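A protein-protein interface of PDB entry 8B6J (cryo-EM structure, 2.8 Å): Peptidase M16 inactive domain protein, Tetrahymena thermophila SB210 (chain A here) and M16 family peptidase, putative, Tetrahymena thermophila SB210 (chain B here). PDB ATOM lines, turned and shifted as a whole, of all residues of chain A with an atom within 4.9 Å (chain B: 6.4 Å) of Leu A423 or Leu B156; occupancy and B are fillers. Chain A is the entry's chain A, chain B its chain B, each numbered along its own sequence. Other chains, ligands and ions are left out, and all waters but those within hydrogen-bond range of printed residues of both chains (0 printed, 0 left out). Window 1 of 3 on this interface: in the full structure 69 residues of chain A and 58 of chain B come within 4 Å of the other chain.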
ATOM      1  N   PRO A  55       2.374 -13.945 -11.369  1.00  0.00           N
ATOM      2  CA  PRO A  55       2.783 -13.581 -12.730  1.00  0.00           C
ATOM      3  C   PRO A  55       3.522 -14.720 -13.414  1.00  0.00           C
ATOM      4  O   PRO A  55       4.148 -15.562 -12.769  1.00  0.00           O
ATOM      5  CB  PRO A  55       3.699 -12.372 -12.516  1.00  0.00           C
ATOM      6  CG  PRO A  55       3.353 -11.853 -11.172  1.00  0.00           C
ATOM      7  CD  PRO A  55       2.955 -13.042 -10.365  1.00  0.00           C
ATOM      8  N   ALA A  57       6.190 -14.577 -15.128  1.00  0.00           N
ATOM      9  CA  ALA A  57       7.632 -14.485 -14.929  1.00  0.00           C
ATOM     10  C   ALA A  57       8.060 -15.181 -13.643  1.00  0.00           C
ATOM     11  O   ALA A  57       9.094 -15.858 -13.610  1.00  0.00           O
ATOM     12  CB  ALA A  57       8.064 -13.019 -14.913  1.00  0.00           C
ATOM     13  N   LEU A  58       7.280 -15.027 -12.574  1.00  0.00           N
ATOM     14  CA  LEU A  58       7.623 -15.618 -11.287  1.00  0.00           C
ATOM     15  C   LEU A  58       7.313 -17.106 -11.211  1.00  0.00           C
ATOM     16  O   LEU A  58       7.649 -17.738 -10.204  1.00  0.00           O
ATOM     17  CB  LEU A  58       6.886 -14.887 -10.163  1.00  0.00           C
ATOM     18  CG  LEU A  58       7.431 -13.503  -9.809  1.00  0.00           C
ATOM     19  CD1 LEU A  58       6.460 -12.757  -8.916  1.00  0.00           C
ATOM     20  CD2 LEU A  58       8.785 -13.617  -9.133  1.00  0.00           C
ATOM     21  N   PHE A 419       6.307  -8.581  -6.044  1.00  0.00           N
ATOM     22  CA  PHE A 419       6.647  -9.289  -7.277  1.00  0.00           C
ATOM     23  C   PHE A 419       7.815  -8.615  -7.988  1.00  0.00           C
ATOM     24  O   PHE A 419       8.753  -9.282  -8.447  1.00  0.00           O
ATOM     25  CB  PHE A 419       5.430  -9.353  -8.204  1.00  0.00           C
ATOM     26  CG  PHE A 419       4.318 -10.238  -7.708  1.00  0.00           C
ATOM     27  CD1 PHE A 419       4.543 -11.209  -6.748  1.00  0.00           C
ATOM     28  CD2 PHE A 419       3.042 -10.100  -8.221  1.00  0.00           C
ATOM     29  CE1 PHE A 419       3.516 -12.017  -6.308  1.00  0.00           C
ATOM     30  CE2 PHE A 419       2.014 -10.906  -7.782  1.00  0.00           C
ATOM     31  CZ  PHE A 419       2.251 -11.864  -6.826  1.00  0.00           C
ATOM     32  N   ASN A 420       7.772  -7.287  -8.094  1.00  0.00           N
ATOM     33  CA  ASN A 420       8.857  -6.575  -8.762  1.00  0.00           C
ATOM     34  C   ASN A 420      10.165  -6.723  -7.996  1.00  0.00           C
ATOM     35  O   ASN A 420      11.232  -6.868  -8.602  1.00  0.00           O
ATOM     36  CB  ASN A 420       8.489  -5.104  -8.936  1.00  0.00           C
ATOM     37  CG  ASN A 420       7.639  -4.861 -10.167  1.00  0.00           C
ATOM     38  OD1 ASN A 420       8.140  -4.439 -11.207  1.00  0.00           O
ATOM     39  ND2 ASN A 420       6.347  -5.142 -10.058  1.00  0.00           N
ATOM     40  N   GLU A 421      10.107  -6.687  -6.663  1.00  0.00           N
ATOM     41  CA  GLU A 421      11.312  -6.897  -5.868  1.00  0.00           C
ATOM     42  C   GLU A 421      11.879  -8.293  -6.090  1.00  0.00           C
ATOM     43  O   GLU A 421      13.098  -8.466  -6.199  1.00  0.00           O
ATOM     44  CB  GLU A 421      11.010  -6.672  -4.388  1.00  0.00           C
ATOM     45  CG  GLU A 421      10.729  -5.226  -4.025  1.00  0.00           C
ATOM     46  CD  GLU A 421      11.958  -4.349  -4.132  1.00  0.00           C
ATOM     47  OE1 GLU A 421      13.053  -4.887  -4.396  1.00  0.00           O
ATOM     48  OE2 GLU A 421      11.831  -3.119  -3.951  1.00  0.00           O
ATOM     49  N   LEU A 422      11.009  -9.303  -6.155  1.00  0.00           N
ATOM     50  CA  LEU A 422      11.475 -10.664  -6.405  1.00  0.00           C
ATOM     51  C   LEU A 422      12.145 -10.772  -7.766  1.00  0.00           C
ATOM     52  O   LEU A 422      13.167 -11.452  -7.911  1.00  0.00           O
ATOM     53  CB  LEU A 422      10.307 -11.647  -6.311  1.00  0.00           C
ATOM     54  CG  LEU A 422       9.731 -11.908  -4.920  1.00  0.00           C
ATOM     55  CD1 LEU A 422       8.490 -12.776  -5.019  1.00  0.00           C
ATOM     56  CD2 LEU A 422      10.766 -12.559  -4.021  1.00  0.00           C
ATOM     57  N   LEU A 423      11.579 -10.119  -8.780  1.00  0.00           N
ATOM     58  CA  LEU A 423      12.154 -10.193 -10.118  1.00  0.00           C
ATOM     59  C   LEU A 423      13.365  -9.287 -10.301  1.00  0.00           C
ATOM     60  O   LEU A 423      14.109  -9.466 -11.270  1.00  0.00           O
ATOM     61  CB  LEU A 423      11.098  -9.837 -11.165  1.00  0.00           C
ATOM     62  CG  LEU A 423       9.891 -10.770 -11.244  1.00  0.00           C
ATOM     63  CD1 LEU A 423       8.861 -10.223 -12.216  1.00  0.00           C
ATOM     64  CD2 LEU A 423      10.322 -12.163 -11.654  1.00  0.00           C
ATOM     65  N   ALA A 424      13.584  -8.328  -9.403  1.00  0.00           N
ATOM     66  CA  ALA A 424      14.615  -7.315  -9.588  1.00  0.00           C
ATOM     67  C   ALA A 424      15.952  -7.672  -8.952  1.00  0.00           C
ATOM     68  O   ALA A 424      16.925  -6.937  -9.149  1.00  0.00           O
ATOM     69  CB  ALA A 424      14.140  -5.973  -9.026  1.00  0.00           C
ATOM     70  N   GLU A 425      16.034  -8.766  -8.196  1.00  0.00           N
ATOM     71  CA  GLU A 425      17.299  -9.179  -7.587  1.00  0.00           C
ATOM     72  C   GLU A 425      18.142  -9.855  -8.662  1.00  0.00           C
ATOM     73  O   GLU A 425      18.114 -11.074  -8.838  1.00  0.00           O
ATOM     74  CB  GLU A 425      17.059 -10.097  -6.394  1.00  0.00           C
ATOM     75  CG  GLU A 425      16.091 -11.244  -6.646  1.00  0.00           C
ATOM     76  CD  GLU A 425      16.072 -12.249  -5.512  1.00  0.00           C
ATOM     77  OE1 GLU A 425      17.043 -12.282  -4.728  1.00  0.00           O
ATOM     78  OE2 GLU A 425      15.084 -13.006  -5.404  1.00  0.00           O
ATOM     79  N   GLN A 426      18.909  -9.043  -9.393  1.00  0.00           N
ATOM     80  CA  GLN A 426      19.675  -9.515 -10.535  1.00  0.00           C
ATOM     81  C   GLN A 426      21.183  -9.406 -10.361  1.00  0.00           C
ATOM     82  O   GLN A 426      21.919  -9.948 -11.192  1.00  0.00           O
ATOM     83  CB  GLN A 426      19.272  -8.743 -11.800  1.00  0.00           C
ATOM     84  CG  GLN A 426      17.791  -8.817 -12.119  1.00  0.00           C
ATOM     85  CD  GLN A 426      17.414  -7.969 -13.313  1.00  0.00           C
ATOM     86  OE1 GLN A 426      18.261  -7.306 -13.908  1.00  0.00           O
ATOM     87  NE2 GLN A 426      16.136  -7.986 -13.672  1.00  0.00           N
ATOM     88  N   ARG A 448      11.694 -18.140  -5.978  1.00  0.00           N
ATOM     89  CA  ARG A 448      10.824 -17.005  -6.269  1.00  0.00           C
ATOM     90  C   ARG A 448       9.365 -17.429  -6.336  1.00  0.00           C
ATOM     91  O   ARG A 448       8.484 -16.754  -5.786  1.00  0.00           O
ATOM     92  CB  ARG A 448      11.238 -16.363  -7.592  1.00  0.00           C
ATOM     93  CG  ARG A 448      12.540 -15.594  -7.544  1.00  0.00           C
ATOM     94  CD  ARG A 448      13.137 -15.427  -8.935  1.00  0.00           C
ATOM     95  NE  ARG A 448      12.123 -15.269  -9.971  1.00  0.00           N
ATOM     96  CZ  ARG A 448      12.391 -15.042 -11.249  1.00  0.00           C
ATOM     97  NH1 ARG A 448      13.632 -14.894 -11.679  1.00  0.00           N
ATOM     98  NH2 ARG A 448      11.388 -14.957 -12.118  1.00  0.00           N
ATOM     99  N   PRO B  86      13.031 -15.306 -17.507  1.00  0.00           N
ATOM    100  CA  PRO B  86      11.795 -14.589 -17.164  1.00  0.00           C
ATOM    101  C   PRO B  86      11.983 -13.593 -16.032  1.00  0.00           C
ATOM    102  O   PRO B  86      12.282 -13.973 -14.896  1.00  0.00           O
ATOM    103  CB  PRO B  86      10.838 -15.718 -16.767  1.00  0.00           C
ATOM    104  CG  PRO B  86      11.314 -16.889 -17.537  1.00  0.00           C
ATOM    105  CD  PRO B  86      12.808 -16.759 -17.616  1.00  0.00           C
ATOM    106  N   SER B  87      11.807 -12.310 -16.339  1.00  0.00           N
ATOM    107  CA  SER B  87      11.970 -11.246 -15.360  1.00  0.00           C
ATOM    108  C   SER B  87      11.130 -10.057 -15.801  1.00  0.00           C
ATOM    109  O   SER B  87      10.479 -10.085 -16.850  1.00  0.00           O
ATOM    110  CB  SER B  87      13.443 -10.862 -15.205  1.00  0.00           C
ATOM    111  OG  SER B  87      13.978 -10.395 -16.430  1.00  0.00           O
ATOM    112  N   GLN B  88      11.144  -9.005 -14.990  1.00  0.00           N
ATOM    113  CA  GLN B  88      10.360  -7.821 -15.305  1.00  0.00           C
ATOM    114  C   GLN B  88      10.888  -7.153 -16.567  1.00  0.00           C
ATOM    115  O   GLN B  88      12.099  -7.023 -16.764  1.00  0.00           O
ATOM    116  CB  GLN B  88      10.381  -6.837 -14.136  1.00  0.00           C
ATOM    117  CG  GLN B  88      11.753  -6.298 -13.783  1.00  0.00           C
ATOM    118  CD  GLN B  88      11.696  -5.272 -12.671  1.00  0.00           C
ATOM    119  OE1 GLN B  88      10.645  -5.049 -12.072  1.00  0.00           O
ATOM    120  NE2 GLN B  88      12.827  -4.639 -12.392  1.00  0.00           N
ATOM    121  N   VAL B  89       9.969  -6.733 -17.425  1.00  0.00           N
ATOM    122  CA  VAL B  89      10.323  -6.081 -18.678  1.00  0.00           C
ATOM    123  C   VAL B  89      10.737  -4.645 -18.400  1.00  0.00           C
ATOM    124  O   VAL B  89      10.102  -3.935 -17.602  1.00  0.00           O
ATOM    125  CB  VAL B  89       9.144  -6.138 -19.666  1.00  0.00           C
ATOM    126  CG1 VAL B  89       9.510  -5.456 -20.974  1.00  0.00           C
ATOM    127  CG2 VAL B  89       8.726  -7.578 -19.911  1.00  0.00           C
ATOM    128  N   MET B  91      11.660  -0.874 -20.254  1.00  0.00           N
ATOM    129  CA  MET B  91      11.425  -0.071 -21.441  1.00  0.00           C
ATOM    130  C   MET B  91      12.060   1.294 -21.230  1.00  0.00           C
ATOM    131  O   MET B  91      12.313   1.713 -20.100  1.00  0.00           O
ATOM    132  CB  MET B  91       9.927   0.076 -21.734  1.00  0.00           C
ATOM    133  CG  MET B  91       9.217  -1.246 -21.978  1.00  0.00           C
ATOM    134  SD  MET B  91       7.422  -1.102 -21.966  1.00  0.00           S
ATOM    135  CE  MET B  91       7.128  -0.675 -20.251  1.00  0.00           C
ATOM    136  N   SER B 136       1.492  -0.696 -10.717  1.00  0.00           N
ATOM    137  CA  SER B 136       2.230  -1.684 -11.494  1.00  0.00           C
ATOM    138  C   SER B 136       3.302  -2.368 -10.661  1.00  0.00           C
ATOM    139  O   SER B 136       3.748  -3.461 -11.022  1.00  0.00           O
ATOM    140  CB  SER B 136       2.868  -1.025 -12.715  1.00  0.00           C
ATOM    141  OG  SER B 136       3.878  -0.113 -12.327  1.00  0.00           O
ATOM    142  N   GLY B 138       6.328  -1.466 -10.398  1.00  0.00           N
ATOM    143  CA  GLY B 138       7.628  -1.160 -10.958  1.00  0.00           C
ATOM    144  C   GLY B 138       8.053   0.259 -10.666  1.00  0.00           C
ATOM    145  O   GLY B 138       7.667   0.854  -9.657  1.00  0.00           O
ATOM    146  N   ASN B 154      10.453   0.191 -15.588  1.00  0.00           N
ATOM    147  CA  ASN B 154      10.487  -1.258 -15.457  1.00  0.00           C
ATOM    148  C   ASN B 154       9.208  -1.707 -14.777  1.00  0.00           C
ATOM    149  O   ASN B 154       8.728  -1.045 -13.851  1.00  0.00           O
ATOM    150  CB  ASN B 154      11.712  -1.722 -14.661  1.00  0.00           C
ATOM    151  CG  ASN B 154      11.921  -0.923 -13.393  1.00  0.00           C
ATOM    152  OD1 ASN B 154      10.989  -0.321 -12.864  1.00  0.00           O
ATOM    153  ND2 ASN B 154      13.153  -0.909 -12.901  1.00  0.00           N
ATOM    154  N   CYS B 155       8.652  -2.823 -15.241  1.00  0.00           N
ATOM    155  CA  CYS B 155       7.378  -3.299 -14.709  1.00  0.00           C
ATOM    156  C   CYS B 155       7.178  -4.746 -15.142  1.00  0.00           C
ATOM    157  O   CYS B 155       7.991  -5.316 -15.873  1.00  0.00           O
ATOM    158  CB  CYS B 155       6.221  -2.417 -15.179  1.00  0.00           C
ATOM    159  SG  CYS B 155       6.029  -2.353 -16.973  1.00  0.00           S
ATOM    160  N   LEU B 156       6.081  -5.336 -14.676  1.00  0.00           N
ATOM    161  CA  LEU B 156       5.719  -6.684 -15.080  1.00  0.00           C
ATOM    162  C   LEU B 156       5.260  -6.694 -16.535  1.00  0.00           C
ATOM    163  O   LEU B 156       4.847  -5.675 -17.093  1.00  0.00           O
ATOM    164  CB  LEU B 156       4.613  -7.237 -14.180  1.00  0.00           C
ATOM    165  CG  LEU B 156       4.956  -7.367 -12.695  1.00  0.00           C
ATOM    166  CD1 LEU B 156       3.730  -7.776 -11.897  1.00  0.00           C
ATOM    167  CD2 LEU B 156       6.082  -8.364 -12.490  1.00  0.00           C
ATOM    168  N   ALA B 157       5.338  -7.873 -17.151  1.00  0.00           N
ATOM    169  CA  ALA B 157       4.980  -7.991 -18.560  1.00  0.00           C
ATOM    170  C   ALA B 157       3.524  -7.609 -18.794  1.00  0.00           C
ATOM    171  O   ALA B 157       3.211  -6.839 -19.708  1.00  0.00           O
ATOM    172  CB  ALA B 157       5.248  -9.413 -19.050  1.00  0.00           C
ATOM    173  N   HIS B 158       2.616  -8.127 -17.964  1.00  0.00           N
ATOM    174  CA  HIS B 158       1.196  -7.894 -18.192  1.00  0.00           C
ATOM    175  C   HIS B 158       0.803  -6.437 -17.986  1.00  0.00           C
ATOM    176  O   HIS B 158      -0.266  -6.027 -18.449  1.00  0.00           O
ATOM    177  CB  HIS B 158       0.358  -8.797 -17.282  1.00  0.00           C
ATOM    178  CG  HIS B 158       0.615  -8.599 -15.821  1.00  0.00           C
ATOM    179  ND1 HIS B 158       0.203  -7.476 -15.137  1.00  0.00           N
ATOM    180  CD2 HIS B 158       1.231  -9.389 -14.911  1.00  0.00           C
ATOM    181  CE1 HIS B 158       0.560  -7.580 -13.869  1.00  0.00           C
ATOM    182  NE2 HIS B 158       1.185  -8.732 -13.706  1.00  0.00           N
ATOM    183  N   ASP B 159       1.635  -5.648 -17.308  1.00  0.00           N
ATOM    184  CA  ASP B 159       1.406  -4.219 -17.152  1.00  0.00           C
ATOM    185  C   ASP B 159       2.253  -3.386 -18.105  1.00  0.00           C
ATOM    186  O   ASP B 159       2.229  -2.155 -18.022  1.00  0.00           O
ATOM    187  CB  ASP B 159       1.686  -3.794 -15.709  1.00  0.00           C
ATOM    188  CG  ASP B 159       0.700  -4.387 -14.725  1.00  0.00           C
ATOM    189  OD1 ASP B 159      -0.474  -4.585 -15.102  1.00  0.00           O
ATOM    190  OD2 ASP B 159       1.097  -4.655 -13.571  1.00  0.00           O
ATOM    191  N   ALA B 160       2.996  -4.026 -19.010  1.00  0.00           N
ATOM    192  CA  ALA B 160       3.908  -3.286 -19.874  1.00  0.00           C
ATOM    193  C   ALA B 160       3.151  -2.311 -20.768  1.00  0.00           C
ATOM    194  O   ALA B 160       3.460  -1.113 -20.798  1.00  0.00           O
ATOM    195  CB  ALA B 160       4.730  -4.258 -20.719  1.00  0.00           C
ATOM    196  N   THR B 161       2.142  -2.805 -21.486  1.00  0.00           N
ATOM    197  CA  THR B 161       1.438  -1.980 -22.463  1.00  0.00           C
ATOM    198  C   THR B 161       1.050  -0.633 -21.866  1.00  0.00           C
ATOM    199  O   THR B 161       1.516   0.420 -22.316  1.00  0.00           O
ATOM    200  CB  THR B 161       0.197  -2.720 -22.968  1.00  0.00           C
ATOM    201  OG1 THR B 161       0.590  -3.955 -23.581  1.00  0.00           O
ATOM    202  CG2 THR B 161      -0.557  -1.874 -23.980  1.00  0.00           C
ATOM    203  N   VAL B 163       1.993   0.856 -19.199  1.00  0.00           N
ATOM    204  CA  VAL B 163       3.150   1.636 -18.770  1.00  0.00           C
ATOM    205  C   VAL B 163       3.786   2.333 -19.963  1.00  0.00           C
ATOM    206  O   VAL B 163       4.158   3.509 -19.884  1.00  0.00           O
ATOM    207  CB  VAL B 163       4.157   0.740 -18.028  1.00  0.00           C
ATOM    208  CG1 VAL B 163       5.489   1.450 -17.875  1.00  0.00           C
ATOM    209  CG2 VAL B 163       3.606   0.352 -16.666  1.00  0.00           C
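OG of Ser B136 lies close to N of Gly B138 (3.4 Å).
N of Val B89 lies within hydrogen-bond range of O of Cys B155, 2.9 Å away.
O of Ala A57 sits at hydrogen-bond distance from NH2 of Arg A448 (2.9 Å).
O of Leu A423 is in hydrogen-bond range of NE2 of Gln A426.
Of chain B, only Gln B88 and Leu B156 come within 4 Å of Leu A423.
Printed residues of chain A within 4 Å of Cys B155: Asn A420.
Printed residues of chain B within 4 Å of Ala A57: Pro B86.
Printed residues of chain B within 4 Å of Arg A448: Pro B86 (3.1 Å).
Of the printed residues of chain A, Gln B88 touches Asn A420 (2.7 Å), Leu A423 (3.8 Å) and Ala A424 (3.9 Å).
Of the printed residues of chain B, Ala A424 touches Gln B88 (3.9 Å).
Phe A419 touches none of the printed residues of chain B.
Leu A58 touches none of the printed residues of chain B.
Among the printed residues, pairs that only touch across the chains: Ala A57 with Pro B86 (3.6 Å), Asn A420 with Gly B138 (3.3 Å), Asn A420 with Cys B155 (3.8 Å), Asn A420 with Leu B156 (3.7 Å), Leu A423 with Gln B88 (3.8 Å), Leu A423 with Leu B156 (3.4 Å) and Ala A424 with Gln B88 (3.9 Å).
O of Ser B136 sits at hydrogen-bond distance from ND2 of Asn A420 (3.2 Å).
NH2 of Arg A448 sits at hydrogen-bond distance from O of Pro B86 (3.1 Å).
OD1 of Asn A420 sits close to OE1 of Gln B88.
Printed residues of chain A that touch a printed residue of chain B: Ala A57, Asn A420, Leu A423, Ala A424 and Arg A448.
Among the printed residues, 10 pairs touch across the chains.
Among the printed residues, no Asp or Glu carboxylate lies within 4 Å of a Lys or Arg side-chain nitrogen of the other chain.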
